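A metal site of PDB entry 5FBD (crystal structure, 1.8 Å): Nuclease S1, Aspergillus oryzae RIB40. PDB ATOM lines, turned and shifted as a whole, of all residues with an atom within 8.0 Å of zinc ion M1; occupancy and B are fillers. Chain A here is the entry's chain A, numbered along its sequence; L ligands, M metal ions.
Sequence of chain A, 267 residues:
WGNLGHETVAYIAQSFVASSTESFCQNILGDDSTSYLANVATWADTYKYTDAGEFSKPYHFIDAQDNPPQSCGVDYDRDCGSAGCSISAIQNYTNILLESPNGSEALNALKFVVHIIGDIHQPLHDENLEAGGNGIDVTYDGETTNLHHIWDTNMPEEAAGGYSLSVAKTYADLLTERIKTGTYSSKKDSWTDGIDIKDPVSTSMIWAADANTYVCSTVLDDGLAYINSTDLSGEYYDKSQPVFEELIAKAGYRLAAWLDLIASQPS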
ATOM      1  N   TRP A   1     -21.401 -27.734  14.465  1.00  0.00           N
ATOM      2  CA  TRP A   1     -21.041 -26.848  13.375  1.00  0.00           C
ATOM      3  C   TRP A   1     -22.010 -25.703  13.425  1.00  0.00           C
ATOM      4  O   TRP A   1     -23.096 -25.845  13.965  1.00  0.00           O
ATOM      5  CB  TRP A   1     -21.137 -27.523  12.002  1.00  0.00           C
ATOM      6  CG  TRP A   1     -20.342 -28.783  11.907  1.00  0.00           C
ATOM      7  CD1 TRP A   1     -20.828 -30.042  11.976  1.00  0.00           C
ATOM      8  CD2 TRP A   1     -18.916 -28.892  11.835  1.00  0.00           C
ATOM      9  NE1 TRP A   1     -19.798 -30.947  11.864  1.00  0.00           N
ATOM     10  CE2 TRP A   1     -18.615 -30.269  11.763  1.00  0.00           C
ATOM     11  CE3 TRP A   1     -17.867 -27.955  11.757  1.00  0.00           C
ATOM     12  CZ2 TRP A   1     -17.310 -30.754  11.721  1.00  0.00           C
ATOM     13  CZ3 TRP A   1     -16.585 -28.411  11.668  1.00  0.00           C
ATOM     14  CH2 TRP A   1     -16.296 -29.836  11.623  1.00  0.00           C
ATOM     15  N   GLY A   2     -21.642 -24.620  12.782  1.00  0.00           N
ATOM     16  CA  GLY A   2     -22.571 -23.540  12.451  1.00  0.00           C
ATOM     17  C   GLY A   2     -23.412 -24.000  11.291  1.00  0.00           C
ATOM     18  O   GLY A   2     -23.318 -25.153  10.805  1.00  0.00           O
ATOM     19  N   HIS A   6     -23.580 -27.626   8.924  1.00  0.00           N
ATOM     20  CA  HIS A   6     -24.710 -28.552   8.971  1.00  0.00           C
ATOM     21  C   HIS A   6     -25.342 -28.757   7.604  1.00  0.00           C
ATOM     22  O   HIS A   6     -25.775 -29.884   7.264  1.00  0.00           O
ATOM     23  CB  HIS A   6     -25.772 -28.071   9.958  1.00  0.00           C
ATOM     24  CG  HIS A   6     -25.372 -28.331  11.372  1.00  0.00           C
ATOM     25  ND1 HIS A   6     -25.315 -29.604  11.887  1.00  0.00           N
ATOM     26  CD2 HIS A   6     -24.914 -27.499  12.350  1.00  0.00           C
ATOM     27  CE1 HIS A   6     -24.842 -29.562  13.132  1.00  0.00           C
ATOM     28  NE2 HIS A   6     -24.552 -28.299  13.415  1.00  0.00           N
ATOM     29  N   ASP A  45     -30.769 -26.266  16.325  1.00  0.00           N
ATOM     30  CA  ASP A  45     -29.954 -25.236  16.994  1.00  0.00           C
ATOM     31  C   ASP A  45     -30.733 -24.025  17.410  1.00  0.00           C
ATOM     32  O   ASP A  45     -30.363 -23.378  18.345  1.00  0.00           O
ATOM     33  CB  ASP A  45     -28.740 -24.822  16.153  1.00  0.00           C
ATOM     34  CG  ASP A  45     -27.541 -25.717  16.382  1.00  0.00           C
ATOM     35  OD1 ASP A  45     -27.546 -26.570  17.343  1.00  0.00           O
ATOM     36  OD2 ASP A  45     -26.593 -25.594  15.586  1.00  0.00           O
ATOM     37  N   LYS A  48     -33.630 -25.586  20.370  1.00  0.00           N
ATOM     38  CA  LYS A  48     -33.154 -25.756  21.725  1.00  0.00           C
ATOM     39  C   LYS A  48     -33.201 -24.547  22.629  1.00  0.00           C
ATOM     40  O   LYS A  48     -33.023 -24.692  23.857  1.00  0.00           O
ATOM     41  CB  LYS A  48     -31.731 -26.319  21.756  1.00  0.00           C
ATOM     42  CG  LYS A  48     -30.643 -25.346  21.269  1.00  0.00           C
ATOM     43  CD  LYS A  48     -29.376 -26.102  20.977  1.00  0.00           C
ATOM     44  CE  LYS A  48     -28.195 -25.217  20.594  1.00  0.00           C
ATOM     45  NZ  LYS A  48     -27.001 -25.993  20.145  1.00  0.00           N
ATOM     46  N   HIS A  60     -26.690 -32.117  21.738  1.00  0.00           N
ATOM     47  CA  HIS A  60     -25.789 -31.661  20.673  1.00  0.00           C
ATOM     48  C   HIS A  60     -24.352 -32.138  20.821  1.00  0.00           C
ATOM     49  O   HIS A  60     -23.524 -31.918  19.909  1.00  0.00           O
ATOM     50  CB  HIS A  60     -25.896 -30.165  20.492  1.00  0.00           C
ATOM     51  CG  HIS A  60     -27.230 -29.728  19.990  1.00  0.00           C
ATOM     52  ND1 HIS A  60     -27.411 -29.159  18.737  1.00  0.00           N
ATOM     53  CD2 HIS A  60     -28.468 -29.859  20.530  1.00  0.00           C
ATOM     54  CE1 HIS A  60     -28.680 -28.856  18.585  1.00  0.00           C
ATOM     55  NE2 HIS A  60     -29.344 -29.352  19.623  1.00  0.00           N
ATOM     56  N   PHE A  61     -24.022 -32.697  21.979  1.00  0.00           N
ATOM     57  CA  PHE A  61     -22.639 -33.029  22.260  1.00  0.00           C
ATOM     58  C   PHE A  61     -22.549 -34.167  23.269  1.00  0.00           C
ATOM     59  O   PHE A  61     -23.565 -34.620  23.845  1.00  0.00           O
ATOM     60  CB  PHE A  61     -21.896 -31.790  22.800  1.00  0.00           C
ATOM     61  CG  PHE A  61     -22.618 -31.119  23.949  1.00  0.00           C
ATOM     62  CD1 PHE A  61     -22.455 -31.559  25.233  1.00  0.00           C
ATOM     63  CD2 PHE A  61     -23.482 -30.086  23.709  1.00  0.00           C
ATOM     64  CE1 PHE A  61     -23.115 -30.931  26.301  1.00  0.00           C
ATOM     65  CE2 PHE A  61     -24.183 -29.481  24.762  1.00  0.00           C
ATOM     66  CZ  PHE A  61     -23.979 -29.910  26.054  1.00  0.00           C
ATOM     67  N   HIS A 115     -29.112 -33.285  12.003  1.00  0.00           N
ATOM     68  CA  HIS A 115     -28.299 -32.276  12.694  1.00  0.00           C
ATOM     69  C   HIS A 115     -27.196 -32.932  13.551  1.00  0.00           C
ATOM     70  O   HIS A 115     -26.051 -32.493  13.509  1.00  0.00           O
ATOM     71  CB  HIS A 115     -29.181 -31.469  13.661  1.00  0.00           C
ATOM     72  CG  HIS A 115     -28.448 -30.337  14.301  1.00  0.00           C
ATOM     73  ND1 HIS A 115     -28.241 -29.122  13.663  1.00  0.00           N
ATOM     74  CD2 HIS A 115     -27.802 -30.259  15.463  1.00  0.00           C
ATOM     75  CE1 HIS A 115     -27.555 -28.337  14.461  1.00  0.00           C
ATOM     76  NE2 HIS A 115     -27.265 -29.013  15.555  1.00  0.00           N
ATOM     77  N   ASP A 119     -23.130 -32.781  14.219  1.00  0.00           N
ATOM     78  CA  ASP A 119     -22.467 -32.269  15.454  1.00  0.00           C
ATOM     79  C   ASP A 119     -21.455 -33.250  16.015  1.00  0.00           C
ATOM     80  O   ASP A 119     -20.421 -32.851  16.478  1.00  0.00           O
ATOM     81  CB  ASP A 119     -23.490 -31.915  16.556  1.00  0.00           C
ATOM     82  CG  ASP A 119     -23.961 -30.460  16.488  1.00  0.00           C
ATOM     83  OD1 ASP A 119     -23.300 -29.682  15.793  1.00  0.00           O
ATOM     84  OD2 ASP A 119     -24.974 -30.103  17.124  1.00  0.00           O
ATOM     85  N   GLN A 122     -17.914 -32.794  14.808  1.00  0.00           N
ATOM     86  CA  GLN A 122     -17.188 -31.603  15.180  1.00  0.00           C
ATOM     87  C   GLN A 122     -16.425 -32.004  16.482  1.00  0.00           C
ATOM     88  O   GLN A 122     -17.053 -32.281  17.482  1.00  0.00           O
ATOM     89  CB  GLN A 122     -18.128 -30.404  15.400  1.00  0.00           C
ATOM     90  CG  GLN A 122     -17.477 -29.037  15.224  1.00  0.00           C
ATOM     91  CD  GLN A 122     -16.535 -28.618  16.354  1.00  0.00           C
ATOM     92  OE1 GLN A 122     -15.539 -29.315  16.673  1.00  0.00           O
ATOM     93  NE2 GLN A 122     -16.800 -27.461  16.966  1.00  0.00           N
ATOM     94  N   LEU A 124     -14.864 -30.798  18.994  1.00  0.00           N
ATOM     95  CA  LEU A 124     -15.162 -30.164  20.287  1.00  0.00           C
ATOM     96  C   LEU A 124     -16.555 -30.422  20.799  1.00  0.00           C
ATOM     97  O   LEU A 124     -16.844 -30.116  21.937  1.00  0.00           O
ATOM     98  CB  LEU A 124     -14.870 -28.665  20.223  1.00  0.00           C
ATOM     99  CG  LEU A 124     -13.401 -28.309  20.293  1.00  0.00           C
ATOM    100  CD1 LEU A 124     -13.229 -26.810  19.956  1.00  0.00           C
ATOM    101  CD2 LEU A 124     -12.802 -28.594  21.672  1.00  0.00           C
ATOM    102  N   HIS A 125     -17.431 -31.012  19.985  1.00  0.00           N
ATOM    103  CA  HIS A 125     -18.717 -31.567  20.469  1.00  0.00           C
ATOM    104  C   HIS A 125     -18.560 -32.946  21.104  1.00  0.00           C
ATOM    105  O   HIS A 125     -19.560 -33.567  21.505  1.00  0.00           O
ATOM    106  CB  HIS A 125     -19.689 -31.668  19.289  1.00  0.00           C
ATOM    107  CG  HIS A 125     -20.369 -30.370  18.953  1.00  0.00           C
ATOM    108  ND1 HIS A 125     -21.714 -30.171  19.162  1.00  0.00           N
ATOM    109  CD2 HIS A 125     -19.893 -29.205  18.459  1.00  0.00           C
ATOM    110  CE1 HIS A 125     -22.037 -28.933  18.871  1.00  0.00           C
ATOM    111  NE2 HIS A 125     -20.954 -28.334  18.393  1.00  0.00           N
ATOM    112  N   ALA A 131     -16.323 -26.354  28.505  1.00  0.00           N
ATOM    113  CA  ALA A 131     -17.606 -26.415  27.842  1.00  0.00           C
ATOM    114  C   ALA A 131     -17.432 -26.683  26.337  1.00  0.00           C
ATOM    115  O   ALA A 131     -17.980 -25.998  25.519  1.00  0.00           O
ATOM    116  CB  ALA A 131     -18.373 -25.145  28.116  1.00  0.00           C
ATOM    117  N   GLY A 132     -16.652 -27.698  25.963  1.00  0.00           N
ATOM    118  CA  GLY A 132     -16.413 -27.988  24.564  1.00  0.00           C
ATOM    119  C   GLY A 132     -15.621 -26.882  23.891  1.00  0.00           C
ATOM    120  O   GLY A 132     -15.836 -26.581  22.720  1.00  0.00           O
ATOM    121  N   ASN A 134     -15.812 -23.693  24.562  1.00  0.00           N
ATOM    122  CA  ASN A 134     -16.505 -22.391  24.554  1.00  0.00           C
ATOM    123  C   ASN A 134     -15.806 -21.380  25.512  1.00  0.00           C
ATOM    124  O   ASN A 134     -15.834 -20.165  25.276  1.00  0.00           O
ATOM    125  CB  ASN A 134     -17.977 -22.533  24.943  1.00  0.00           C
ATOM    126  CG  ASN A 134     -18.833 -22.925  23.751  1.00  0.00           C
ATOM    127  OD1 ASN A 134     -19.022 -22.134  22.833  1.00  0.00           O
ATOM    128  ND2 ASN A 134     -19.288 -24.166  23.732  1.00  0.00           N
ATOM    129  N   HIS A 148     -14.391 -23.052  20.370  1.00  0.00           N
ATOM    130  CA  HIS A 148     -15.559 -23.719  19.826  1.00  0.00           C
ATOM    131  C   HIS A 148     -16.135 -23.003  18.578  1.00  0.00           C
ATOM    132  O   HIS A 148     -16.402 -23.653  17.533  1.00  0.00           O
ATOM    133  CB  HIS A 148     -16.601 -23.885  20.907  1.00  0.00           C
ATOM    134  CG  HIS A 148     -17.716 -24.805  20.497  1.00  0.00           C
ATOM    135  ND1 HIS A 148     -17.773 -26.127  20.890  1.00  0.00           N
ATOM    136  CD2 HIS A 148     -18.768 -24.618  19.667  1.00  0.00           C
ATOM    137  CE1 HIS A 148     -18.855 -26.679  20.383  1.00  0.00           C
ATOM    138  NE2 HIS A 148     -19.466 -25.794  19.631  1.00  0.00           N
ATOM    139  N   HIS A 149     -16.258 -21.670  18.647  1.00  0.00           N
ATOM    140  CA  HIS A 149     -16.873 -20.873  17.600  1.00  0.00           C
ATOM    141  C   HIS A 149     -16.069 -20.956  16.283  1.00  0.00           C
ATOM    142  O   HIS A 149     -16.612 -21.045  15.161  1.00  0.00           O
ATOM    143  CB  HIS A 149     -17.079 -19.372  18.084  1.00  0.00           C
ATOM    144  CG  HIS A 149     -18.016 -18.565  17.214  1.00  0.00           C
ATOM    145  ND1 HIS A 149     -17.636 -18.054  15.994  1.00  0.00           N
ATOM    146  CD2 HIS A 149     -19.320 -18.227  17.365  1.00  0.00           C
ATOM    147  CE1 HIS A 149     -18.622 -17.374  15.454  1.00  0.00           C
ATOM    148  NE2 HIS A 149     -19.669 -17.505  16.239  1.00  0.00           N
ATOM    149  N   TRP A 151     -14.100 -23.483  15.234  1.00  0.00           N
ATOM    150  CA  TRP A 151     -14.346 -24.828  14.686  1.00  0.00           C
ATOM    151  C   TRP A 151     -15.738 -24.968  14.133  1.00  0.00           C
ATOM    152  O   TRP A 151     -15.921 -25.542  13.082  1.00  0.00           O
ATOM    153  CB  TRP A 151     -14.034 -25.960  15.744  1.00  0.00           C
ATOM    154  CG  TRP A 151     -12.541 -26.240  15.764  1.00  0.00           C
ATOM    155  CD1 TRP A 151     -11.607 -25.565  16.459  1.00  0.00           C
ATOM    156  CD2 TRP A 151     -11.835 -27.200  14.967  1.00  0.00           C
ATOM    157  NE1 TRP A 151     -10.349 -26.072  16.207  1.00  0.00           N
ATOM    158  CE2 TRP A 151     -10.459 -27.079  15.301  1.00  0.00           C
ATOM    159  CE3 TRP A 151     -12.217 -28.158  14.032  1.00  0.00           C
ATOM    160  CZ2 TRP A 151      -9.503 -27.833  14.714  1.00  0.00           C
ATOM    161  CZ3 TRP A 151     -11.249 -28.960  13.469  1.00  0.00           C
ATOM    162  CH2 TRP A 151      -9.895 -28.795  13.799  1.00  0.00           C
ATOM    163  N   ASP A 152     -16.749 -24.402  14.819  1.00  0.00           N
ATOM    164  CA  ASP A 152     -18.097 -24.482  14.303  1.00  0.00           C
ATOM    165  C   ASP A 152     -18.288 -23.632  13.090  1.00  0.00           C
ATOM    166  O   ASP A 152     -18.967 -24.035  12.117  1.00  0.00           O
ATOM    167  CB  ASP A 152     -19.136 -24.014  15.380  1.00  0.00           C
ATOM    168  CG  ASP A 152     -19.733 -25.165  16.190  1.00  0.00           C
ATOM    169  OD1 ASP A 152     -19.312 -26.344  16.125  1.00  0.00           O
ATOM    170  OD2 ASP A 152     -20.669 -24.819  16.884  1.00  0.00           O
ATOM    171  N   THR A 153     -17.735 -22.416  13.134  1.00  0.00           N
ATOM    172  CA  THR A 153     -18.163 -21.342  12.206  1.00  0.00           C
ATOM    173  C   THR A 153     -17.061 -20.650  11.443  1.00  0.00           C
ATOM    174  O   THR A 153     -17.092 -20.702  10.208  1.00  0.00           O
ATOM    175  CB  THR A 153     -19.058 -20.330  12.911  1.00  0.00           C
ATOM    176  OG1 THR A 153     -20.184 -21.051  13.404  1.00  0.00           O
ATOM    177  CG2 THR A 153     -19.506 -19.151  12.014  1.00  0.00           C
HETATM  178  P1  LIG L   1     -23.996 -26.259  17.886  1.00  0.00           P
HETATM  179  O1  LIG L   1     -23.328 -26.546  16.573  1.00  0.00           O
HETATM  180  O2  LIG L   1     -24.942 -27.313  18.407  1.00  0.00           O
HETATM  181  O3  LIG L   1     -22.823 -25.969  18.792  1.00  0.00           O
HETATM  182  O4  LIG L   1     -24.805 -24.956  17.799  1.00  0.00           O
HETATM  183  N1  LG2 L   2     -21.593 -26.991  23.264  1.00  0.00           N
HETATM  184  C1  LG2 L   2     -20.777 -28.124  23.214  1.00  0.00           C
HETATM  185  N2  LG2 L   2     -20.325 -28.653  24.373  1.00  0.00           N
HETATM  186  C2  LG2 L   2     -20.662 -28.074  25.551  1.00  0.00           C
HETATM  187  C3  LG2 L   2     -21.489 -26.924  25.613  1.00  0.00           C
HETATM  188  C4  LG2 L   2     -21.911 -26.423  24.460  1.00  0.00           C
HETATM  189  O1  LG2 L   2     -20.498 -28.614  22.097  1.00  0.00           O
HETATM  190  N3  LG2 L   2     -20.219 -28.614  26.659  1.00  0.00           N
HETATM  191  C5  LG2 L   2     -22.049 -26.393  22.017  1.00  0.00           C
HETATM  192  C6  LG2 L   2     -23.571 -26.266  21.978  1.00  0.00           C
HETATM  193  C7  LG2 L   2     -23.834 -24.766  22.063  1.00  0.00           C
HETATM  194  C8  LG2 L   2     -22.526 -24.128  21.619  1.00  0.00           C
HETATM  195  O2  LG2 L   2     -21.498 -25.077  21.960  1.00  0.00           O
HETATM  196  O3  LG2 L   2     -24.809 -24.454  21.074  1.00  0.00           O
HETATM  197  C9  LG2 L   2     -22.213 -22.784  22.251  1.00  0.00           C
HETATM  198  O4  LG2 L   2     -22.578 -22.762  23.650  1.00  0.00           O
HETATM  199 ZN    ZN M   1     -20.999 -26.267  18.299  1.00  0.00          ZN
HETATM  200 ZN    ZN M   2     -23.378 -27.734  15.025  1.00  0.00          ZN
HETATM  201 ZN    ZN M   3     -26.182 -28.456  17.335  1.00  0.00          ZN
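An oxygen (O2) of LG2 L2 lies close to a ring nitrogen (NE2) of His 148 (3.2 Å). ND2 of Asn 134 sits at hydrogen-bond distance from O2 of LG2 L2. An oxygen (O3) of LG2 L2 is in hydrogen-bond range of the side-chain amino group (NZ) of Lys 48 (2.8 Å).
The side-chain carboxylate (OD1) of Asp 152 lies close to the backbone NH (N) of Trp 1, 3.0 Å away. NE2 of Gln 122 sits at hydrogen-bond distance from OD1 of Asp 152 (2.9 Å). The backbone carbonyl oxygen (O) of Asp 152 is in hydrogen-bond range of the backbone NH (N) of Gly 2 (2.8 Å). ND1 of His 125 lies within hydrogen-bond range of O of His 60. The backbone carbonyl oxygen of Gly 132 is in hydrogen-bond range of a ring nitrogen (ND1) of His 148 (2.7 Å).
Of the 20 residues printed, 3 come within 4 Å of zinc ion M1.
O3 of LIG L1 is bound to zinc ion M1 (1.9 Å). The side-chain carboxylate (OD2) of Asp 152 binds zinc ion M1, at 2.1 Å. NE2 of His 125 binds zinc ion M1 (2.1 Å). Zinc ion M1 is bound by NE2 of His 148 (2.1 Å). Slightly farther from zinc ion M1 lies the side-chain carboxylate (OD1) of Asp 152 (2.8 Å).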
